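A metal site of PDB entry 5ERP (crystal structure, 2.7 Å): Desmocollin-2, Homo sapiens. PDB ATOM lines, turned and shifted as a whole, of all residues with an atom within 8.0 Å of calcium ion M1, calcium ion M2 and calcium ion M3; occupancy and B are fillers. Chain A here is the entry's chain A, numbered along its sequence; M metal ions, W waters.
OE2 of Glu 232 lies close to ND2 of Asn 132 (2.7 Å).
The guanidinium group (NH2) of Arg 322 lies close to the backbone carbonyl oxygen (O) of Glu 232 (3.4 Å).
OG1 of Thr 265 lies close to OD2 of Asp 262, 3.1 Å away.
NH2 of Arg 322 lies within salt-bridge range of OD2 of Asp 231 (3.6 Å).
The backbone NH (N) of Tyr 190 lies close to the side-chain carboxylate (OE1) of Glu 131.
The backbone NH of Glu 131 sits at hydrogen-bond distance from the backbone carbonyl oxygen of Glu 228 (3.1 Å).
The backbone NH of Asn 132 is in hydrogen-bond range of the backbone carbonyl oxygen of Leu 188, at 2.8 Å.
The guanidinium group (NE) of Arg 322 lies within salt-bridge range of the side-chain carboxylate (OD2) of Asp 318, 3.1 Å away.
ND2 of Asn 132 touches calcium ion M1, 3.6 Å away.
Within 4 Å of calcium ion M1: Glu 131, Asn 132, Asn 189, Glu 191 and Glu 232.
Along chain A the residues within 4 Å of calcium ion M1 span positions 131 to 232.
The nearest printed residue that does not touch calcium ion M1 is Tyr 190 (4.7 Å).
Of the 24 residues printed, 6 come within 4 Å of calcium ion M2.
Arg 322 touches calcium ion M3 (NH2 to CA, 3.9 Å).
Of the 24 residues printed, 5 come within 4 Å of calcium ion M3.
The side-chain amide oxygen (OD1) of Asn 189 binds calcium ion M1 (2.2 Å).
Calcium ion M1 is bound by OE1 of Glu 232 (2.3 Å).
The side-chain carboxylate (OE2) of Glu 232 is bound to calcium ion M1 (2.4 Å).
OE2 of Glu 191 binds calcium ion M1 (2.5 Å).
Calcium ion M1 is bound by water W1 (2.5 Å).
OE1 of Glu 131 is bound to calcium ion M1 (2.6 Å).
Calcium ion M1 has six donor atoms within binding distance.
Calcium ion M2 is bound by OE1 of Glu 232, OE1 of Glu 191, OE2 of Glu 264, OD1 of Asp 229, OE2 of Glu 131 and O of Gln 230.
Calcium ion M3 is bound by the side-chain carboxylate (OD1) of Asp 262.
The side-chain carboxylate (OD1) of Asp 231 binds calcium ion M3 (2.3 Å).
OE1 of Glu 264 is bound to calcium ion M3 (2.4 Å).
The backbone carbonyl oxygen (O) of Glu 232 binds calcium ion M3, at 2.6 Å.
OD2 of Asp 262 binds calcium ion M3, at 2.6 Å.
Water W2 binds calcium ion M3 (2.7 Å).
Calcium ion M3 has six donor atoms within binding distance.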
ATOM      1  N   GLU A 131     -14.132  14.943  32.548  1.00  0.00           N
ATOM      2  CA  GLU A 131     -14.560  15.195  31.164  1.00  0.00           C
ATOM      3  C   GLU A 131     -15.392  16.468  31.054  1.00  0.00           C
ATOM      4  O   GLU A 131     -15.896  16.982  32.052  1.00  0.00           O
ATOM      5  CB  GLU A 131     -15.362  14.002  30.629  1.00  0.00           C
ATOM      6  CG  GLU A 131     -16.706  13.795  31.313  1.00  0.00           C
ATOM      7  CD  GLU A 131     -17.507  12.682  30.677  1.00  0.00           C
ATOM      8  OE1 GLU A 131     -17.480  12.569  29.432  1.00  0.00           O
ATOM      9  OE2 GLU A 131     -18.144  11.921  31.423  1.00  0.00           O
ATOM     10  N   ASN A 132     -15.518  16.971  29.825  1.00  0.00           N
ATOM     11  CA  ASN A 132     -16.285  18.175  29.547  1.00  0.00           C
ATOM     12  C   ASN A 132     -15.830  19.342  30.415  1.00  0.00           C
ATOM     13  O   ASN A 132     -16.594  20.248  30.723  1.00  0.00           O
ATOM     14  CB  ASN A 132     -17.776  17.911  29.763  1.00  0.00           C
ATOM     15  CG  ASN A 132     -18.305  16.823  28.854  1.00  0.00           C
ATOM     16  OD1 ASN A 132     -18.113  16.864  27.642  1.00  0.00           O
ATOM     17  ND2 ASN A 132     -18.937  15.817  29.447  1.00  0.00           N
ATOM     18  N   LEU A 188     -12.598  16.959  27.123  1.00  0.00           N
ATOM     19  CA  LEU A 188     -12.434  15.550  26.806  1.00  0.00           C
ATOM     20  C   LEU A 188     -13.755  14.832  27.014  1.00  0.00           C
ATOM     21  O   LEU A 188     -14.636  15.334  27.701  1.00  0.00           O
ATOM     22  CB  LEU A 188     -11.335  14.938  27.672  1.00  0.00           C
ATOM     23  CG  LEU A 188      -9.983  15.655  27.542  1.00  0.00           C
ATOM     24  CD1 LEU A 188      -9.089  15.375  28.734  1.00  0.00           C
ATOM     25  CD2 LEU A 188      -9.299  15.224  26.247  1.00  0.00           C
ATOM     26  N   ASN A 189     -13.877  13.656  26.407  1.00  0.00           N
ATOM     27  CA  ASN A 189     -15.102  12.880  26.490  1.00  0.00           C
ATOM     28  C   ASN A 189     -14.804  11.447  26.894  1.00  0.00           C
ATOM     29  O   ASN A 189     -14.267  10.681  26.101  1.00  0.00           O
ATOM     30  CB  ASN A 189     -15.835  12.909  25.143  1.00  0.00           C
ATOM     31  CG  ASN A 189     -17.283  12.481  25.265  1.00  0.00           C
ATOM     32  OD1 ASN A 189     -17.957  12.843  26.221  1.00  0.00           O
ATOM     33  ND2 ASN A 189     -17.761  11.695  24.318  1.00  0.00           N
ATOM     34  N   TYR A 190     -15.145  11.093  28.130  1.00  0.00           N
ATOM     35  CA  TYR A 190     -14.842   9.766  28.656  1.00  0.00           C
ATOM     36  C   TYR A 190     -15.385   8.653  27.749  1.00  0.00           C
ATOM     37  O   TYR A 190     -14.882   7.533  27.767  1.00  0.00           O
ATOM     38  CB  TYR A 190     -15.397   9.606  30.065  1.00  0.00           C
ATOM     39  CG  TYR A 190     -15.223   8.218  30.644  1.00  0.00           C
ATOM     40  CD1 TYR A 190     -14.037   7.833  31.248  1.00  0.00           C
ATOM     41  CD2 TYR A 190     -16.257   7.280  30.577  1.00  0.00           C
ATOM     42  CE1 TYR A 190     -13.867   6.564  31.765  1.00  0.00           C
ATOM     43  CE2 TYR A 190     -16.102   6.010  31.089  1.00  0.00           C
ATOM     44  CZ  TYR A 190     -14.906   5.652  31.683  1.00  0.00           C
ATOM     45  OH  TYR A 190     -14.738   4.392  32.203  1.00  0.00           O
ATOM     46  N   GLU A 191     -16.416   8.966  26.967  1.00  0.00           N
ATOM     47  CA  GLU A 191     -17.060   7.959  26.139  1.00  0.00           C
ATOM     48  C   GLU A 191     -16.310   7.693  24.834  1.00  0.00           C
ATOM     49  O   GLU A 191     -16.476   6.639  24.226  1.00  0.00           O
ATOM     50  CB  GLU A 191     -18.494   8.388  25.836  1.00  0.00           C
ATOM     51  CG  GLU A 191     -19.454   8.106  26.984  1.00  0.00           C
ATOM     52  CD  GLU A 191     -19.382   9.145  28.096  1.00  0.00           C
ATOM     53  OE1 GLU A 191     -19.785   8.817  29.232  1.00  0.00           O
ATOM     54  OE2 GLU A 191     -18.904  10.270  27.848  1.00  0.00           O
ATOM     55  N   GLU A 192     -15.481   8.645  24.417  1.00  0.00           N
ATOM     56  CA  GLU A 192     -14.626   8.455  23.247  1.00  0.00           C
ATOM     57  C   GLU A 192     -13.297   7.844  23.678  1.00  0.00           C
ATOM     58  O   GLU A 192     -12.899   6.785  23.186  1.00  0.00           O
ATOM     59  CB  GLU A 192     -14.388   9.768  22.522  1.00  0.00           C
ATOM     60  CG  GLU A 192     -13.478   9.649  21.300  1.00  0.00           C
ATOM     61  CD  GLU A 192     -13.321  10.948  20.550  1.00  0.00           C
ATOM     62  OE1 GLU A 192     -12.653  10.947  19.487  1.00  0.00           O
ATOM     63  OE2 GLU A 192     -13.850  11.973  21.019  1.00  0.00           O
ATOM     64  N   VAL A 227      -9.085  10.161  31.913  1.00  0.00           N
ATOM     65  CA  VAL A 227     -10.308  10.954  31.887  1.00  0.00           C
ATOM     66  C   VAL A 227     -11.313  10.398  32.883  1.00  0.00           C
ATOM     67  O   VAL A 227     -11.515   9.191  32.947  1.00  0.00           O
ATOM     68  CB  VAL A 227     -10.929  10.979  30.481  1.00  0.00           C
ATOM     69  CG1 VAL A 227     -12.130  11.905  30.452  1.00  0.00           C
ATOM     70  CG2 VAL A 227      -9.904  11.404  29.438  1.00  0.00           C
ATOM     71  N   GLU A 228     -11.921  11.285  33.668  1.00  0.00           N
ATOM     72  CA  GLU A 228     -12.954  10.888  34.626  1.00  0.00           C
ATOM     73  C   GLU A 228     -14.337  10.993  34.024  1.00  0.00           C
ATOM     74  O   GLU A 228     -14.655  11.954  33.315  1.00  0.00           O
ATOM     75  CB  GLU A 228     -12.900  11.724  35.902  1.00  0.00           C
ATOM     76  CG  GLU A 228     -11.950  11.222  36.963  1.00  0.00           C
ATOM     77  CD  GLU A 228     -12.066  12.016  38.249  1.00  0.00           C
ATOM     78  OE1 GLU A 228     -12.071  13.266  38.182  1.00  0.00           O
ATOM     79  OE2 GLU A 228     -12.156  11.393  39.330  1.00  0.00           O
ATOM     80  N   ASP A 229     -15.168   9.998  34.322  1.00  0.00           N
ATOM     81  CA  ASP A 229     -16.534   9.951  33.850  1.00  0.00           C
ATOM     82  C   ASP A 229     -17.448  10.859  34.677  1.00  0.00           C
ATOM     83  O   ASP A 229     -17.440  10.797  35.915  1.00  0.00           O
ATOM     84  CB  ASP A 229     -17.044   8.499  33.887  1.00  0.00           C
ATOM     85  CG  ASP A 229     -18.423   8.340  33.273  1.00  0.00           C
ATOM     86  OD1 ASP A 229     -18.918   9.295  32.650  1.00  0.00           O
ATOM     87  OD2 ASP A 229     -19.010   7.253  33.430  1.00  0.00           O
ATOM     88  N   GLN A 230     -18.220  11.695  33.991  1.00  0.00           N
ATOM     89  CA  GLN A 230     -19.308  12.438  34.605  1.00  0.00           C
ATOM     90  C   GLN A 230     -20.631  11.776  34.272  1.00  0.00           C
ATOM     91  O   GLN A 230     -20.837  11.348  33.139  1.00  0.00           O
ATOM     92  CB  GLN A 230     -19.358  13.885  34.097  1.00  0.00           C
ATOM     93  CG  GLN A 230     -18.348  14.850  34.670  1.00  0.00           C
ATOM     94  CD  GLN A 230     -18.541  16.251  34.107  1.00  0.00           C
ATOM     95  OE1 GLN A 230     -19.122  16.421  33.028  1.00  0.00           O
ATOM     96  NE2 GLN A 230     -18.085  17.250  34.845  1.00  0.00           N
ATOM     97  N   ASP A 231     -21.535  11.707  35.247  1.00  0.00           N
ATOM     98  CA  ASP A 231     -22.873  11.199  34.988  1.00  0.00           C
ATOM     99  C   ASP A 231     -23.620  12.263  34.189  1.00  0.00           C
ATOM    100  O   ASP A 231     -24.132  13.229  34.740  1.00  0.00           O
ATOM    101  CB  ASP A 231     -23.603  10.876  36.295  1.00  0.00           C
ATOM    102  CG  ASP A 231     -24.975  10.285  36.072  1.00  0.00           C
ATOM    103  OD1 ASP A 231     -25.292   9.918  34.928  1.00  0.00           O
ATOM    104  OD2 ASP A 231     -25.740  10.179  37.059  1.00  0.00           O
ATOM    105  N   GLU A 232     -23.686  12.065  32.870  1.00  0.00           N
ATOM    106  CA  GLU A 232     -24.280  13.058  31.980  1.00  0.00           C
ATOM    107  C   GLU A 232     -25.747  12.767  31.689  1.00  0.00           C
ATOM    108  O   GLU A 232     -26.245  11.679  31.947  1.00  0.00           O
ATOM    109  CB  GLU A 232     -23.488  13.126  30.663  1.00  0.00           C
ATOM    110  CG  GLU A 232     -22.075  13.657  30.833  1.00  0.00           C
ATOM    111  CD  GLU A 232     -21.200  13.324  29.649  1.00  0.00           C
ATOM    112  OE1 GLU A 232     -20.745  12.172  29.556  1.00  0.00           O
ATOM    113  OE2 GLU A 232     -20.968  14.233  28.822  1.00  0.00           O
ATOM    114  N   GLY A 233     -26.425  13.765  31.132  1.00  0.00           N
ATOM    115  CA  GLY A 233     -27.832  13.674  30.820  1.00  0.00           C
ATOM    116  C   GLY A 233     -28.105  13.060  29.462  1.00  0.00           C
ATOM    117  O   GLY A 233     -27.164  12.654  28.774  1.00  0.00           O
ATOM    118  N   PRO A 234     -29.373  13.012  29.062  1.00  0.00           N
ATOM    119  CA  PRO A 234     -29.809  12.347  27.830  1.00  0.00           C
ATOM    120  C   PRO A 234     -29.204  12.983  26.586  1.00  0.00           C
ATOM    121  O   PRO A 234     -28.985  14.185  26.571  1.00  0.00           O
ATOM    122  CB  PRO A 234     -31.331  12.514  27.852  1.00  0.00           C
ATOM    123  CG  PRO A 234     -31.560  13.735  28.656  1.00  0.00           C
ATOM    124  CD  PRO A 234     -30.481  13.744  29.698  1.00  0.00           C
ATOM    125  N   GLU A 235     -28.933  12.158  25.570  1.00  0.00           N
ATOM    126  CA  GLU A 235     -28.347  12.642  24.322  1.00  0.00           C
ATOM    127  C   GLU A 235     -29.281  12.401  23.153  1.00  0.00           C
ATOM    128  O   GLU A 235     -29.846  11.306  23.015  1.00  0.00           O
ATOM    129  CB  GLU A 235     -26.997  11.933  24.085  1.00  0.00           C
ATOM    130  CG  GLU A 235     -26.267  12.341  22.812  1.00  0.00           C
ATOM    131  CD  GLU A 235     -24.911  11.671  22.678  1.00  0.00           C
ATOM    132  OE1 GLU A 235     -24.531  10.889  23.577  1.00  0.00           O
ATOM    133  OE2 GLU A 235     -24.221  11.914  21.665  1.00  0.00           O
ATOM    134  N   TYR A 261     -30.995   8.635  24.466  1.00  0.00           N
ATOM    135  CA  TYR A 261     -30.380   7.644  25.331  1.00  0.00           C
ATOM    136  C   TYR A 261     -29.415   8.275  26.330  1.00  0.00           C
ATOM    137  O   TYR A 261     -28.993   9.420  26.147  1.00  0.00           O
ATOM    138  CB  TYR A 261     -29.659   6.590  24.491  1.00  0.00           C
ATOM    139  CG  TYR A 261     -28.577   7.135  23.589  1.00  0.00           C
ATOM    140  CD1 TYR A 261     -27.299   7.380  24.072  1.00  0.00           C
ATOM    141  CD2 TYR A 261     -28.833   7.400  22.246  1.00  0.00           C
ATOM    142  CE1 TYR A 261     -26.309   7.870  23.250  1.00  0.00           C
ATOM    143  CE2 TYR A 261     -27.849   7.902  21.419  1.00  0.00           C
ATOM    144  CZ  TYR A 261     -26.592   8.136  21.924  1.00  0.00           C
ATOM    145  OH  TYR A 261     -25.603   8.635  21.105  1.00  0.00           O
ATOM    146  N   ASP A 262     -29.087   7.535  27.382  1.00  0.00           N
ATOM    147  CA  ASP A 262     -28.095   7.977  28.350  1.00  0.00           C
ATOM    148  C   ASP A 262     -26.701   7.640  27.819  1.00  0.00           C
ATOM    149  O   ASP A 262     -26.480   6.527  27.339  1.00  0.00           O
ATOM    150  CB  ASP A 262     -28.348   7.301  29.712  1.00  0.00           C
ATOM    151  CG  ASP A 262     -27.499   7.894  30.822  1.00  0.00           C
ATOM    152  OD1 ASP A 262     -27.276   9.118  30.810  1.00  0.00           O
ATOM    153  OD2 ASP A 262     -27.074   7.133  31.710  1.00  0.00           O
ATOM    154  N   PRO A 263     -25.750   8.585  27.892  1.00  0.00           N
ATOM    155  CA  PRO A 263     -24.408   8.285  27.356  1.00  0.00           C
ATOM    156  C   PRO A 263     -23.709   7.143  28.080  1.00  0.00           C
ATOM    157  O   PRO A 263     -23.014   6.359  27.436  1.00  0.00           O
ATOM    158  CB  PRO A 263     -23.657   9.599  27.566  1.00  0.00           C
ATOM    159  CG  PRO A 263     -24.708  10.640  27.582  1.00  0.00           C
ATOM    160  CD  PRO A 263     -25.874  10.009  28.272  1.00  0.00           C
ATOM    161  N   GLU A 264     -23.882   7.045  29.398  1.00  0.00           N
ATOM    162  CA  GLU A 264     -23.263   5.987  30.183  1.00  0.00           C
ATOM    163  C   GLU A 264     -23.952   4.642  29.937  1.00  0.00           C
ATOM    164  O   GLU A 264     -23.309   3.661  29.576  1.00  0.00           O
ATOM    165  CB  GLU A 264     -23.297   6.322  31.673  1.00  0.00           C
ATOM    166  CG  GLU A 264     -22.435   7.510  32.071  1.00  0.00           C
ATOM    167  CD  GLU A 264     -23.047   8.846  31.706  1.00  0.00           C
ATOM    168  OE1 GLU A 264     -24.285   8.995  31.847  1.00  0.00           O
ATOM    169  OE2 GLU A 264     -22.305   9.748  31.270  1.00  0.00           O
ATOM    170  N   THR A 265     -25.265   4.612  30.151  1.00  0.00           N
ATOM    171  CA  THR A 265     -26.040   3.381  30.085  1.00  0.00           C
ATOM    172  C   THR A 265     -26.355   2.923  28.662  1.00  0.00           C
ATOM    173  O   THR A 265     -26.531   1.737  28.413  1.00  0.00           O
ATOM    174  CB  THR A 265     -27.374   3.527  30.843  1.00  0.00           C
ATOM    175  OG1 THR A 265     -27.128   4.070  32.150  1.00  0.00           O
ATOM    176  CG2 THR A 265     -28.081   2.179  30.982  1.00  0.00           C
ATOM    177  N   ARG A 266     -26.422   3.885  27.734  1.00  0.00           N
ATOM    178  CA  ARG A 266     -26.865   3.626  26.359  1.00  0.00           C
ATOM    179  C   ARG A 266     -28.309   3.116  26.323  1.00  0.00           C
ATOM    180  O   ARG A 266     -28.764   2.580  25.319  1.00  0.00           O
ATOM    181  CB  ARG A 266     -25.940   2.624  25.646  1.00  0.00           C
ATOM    182  CG  ARG A 266     -24.510   3.112  25.467  1.00  0.00           C
ATOM    183  CD  ARG A 266     -24.379   4.159  24.364  1.00  0.00           C
ATOM    184  NE  ARG A 266     -24.695   3.621  23.041  1.00  0.00           N
ATOM    185  CZ  ARG A 266     -24.534   4.296  21.906  1.00  0.00           C
ATOM    186  NH1 ARG A 266     -24.062   5.539  21.924  1.00  0.00           N
ATOM    187  NH2 ARG A 266     -24.842   3.721  20.751  1.00  0.00           N
ATOM    188  N   ASP A 318     -34.276  13.421  31.544  1.00  0.00           N
ATOM    189  CA  ASP A 318     -34.017  12.279  32.400  1.00  0.00           C
ATOM    190  C   ASP A 318     -34.596  12.593  33.767  1.00  0.00           C
ATOM    191  O   ASP A 318     -35.100  13.687  33.997  1.00  0.00           O
ATOM    192  CB  ASP A 318     -32.515  11.962  32.484  1.00  0.00           C
ATOM    193  CG  ASP A 318     -31.685  13.090  33.094  1.00  0.00           C
ATOM    194  OD1 ASP A 318     -32.249  14.123  33.526  1.00  0.00           O
ATOM    195  OD2 ASP A 318     -30.452  12.930  33.159  1.00  0.00           O
ATOM    196  N   ARG A 322     -32.297  17.179  33.622  1.00  0.00           N
ATOM    197  CA  ARG A 322     -31.449  17.737  32.580  1.00  0.00           C
ATOM    198  C   ARG A 322     -31.966  17.301  31.217  1.00  0.00           C
ATOM    199  O   ARG A 322     -32.542  16.219  31.066  1.00  0.00           O
ATOM    200  CB  ARG A 322     -29.973  17.355  32.773  1.00  0.00           C
ATOM    201  CG  ARG A 322     -29.694  15.950  33.269  1.00  0.00           C
ATOM    202  CD  ARG A 322     -28.290  15.868  33.816  1.00  0.00           C
ATOM    203  NE  ARG A 322     -27.824  14.484  33.921  1.00  0.00           N
ATOM    204  CZ  ARG A 322     -28.028  13.694  34.968  1.00  0.00           C
ATOM    205  NH1 ARG A 322     -28.694  14.135  36.036  1.00  0.00           N
ATOM    206  NH2 ARG A 322     -27.556  12.458  34.963  1.00  0.00           N
HETATM  207 CA    CA M   1     -19.502  12.680  27.732  1.00  0.00          CA
HETATM  208 CA    CA M   2     -20.066  10.432  30.911  1.00  0.00          CA
HETATM  209 CA    CA M   3     -26.394   9.308  32.956  1.00  0.00          CA
HETATM  210  O   HOH W   1     -21.151  11.966  25.981  1.00  0.00           O
HETATM  211  O   HOH W   2     -26.268   7.056  34.379  1.00  0.00           O
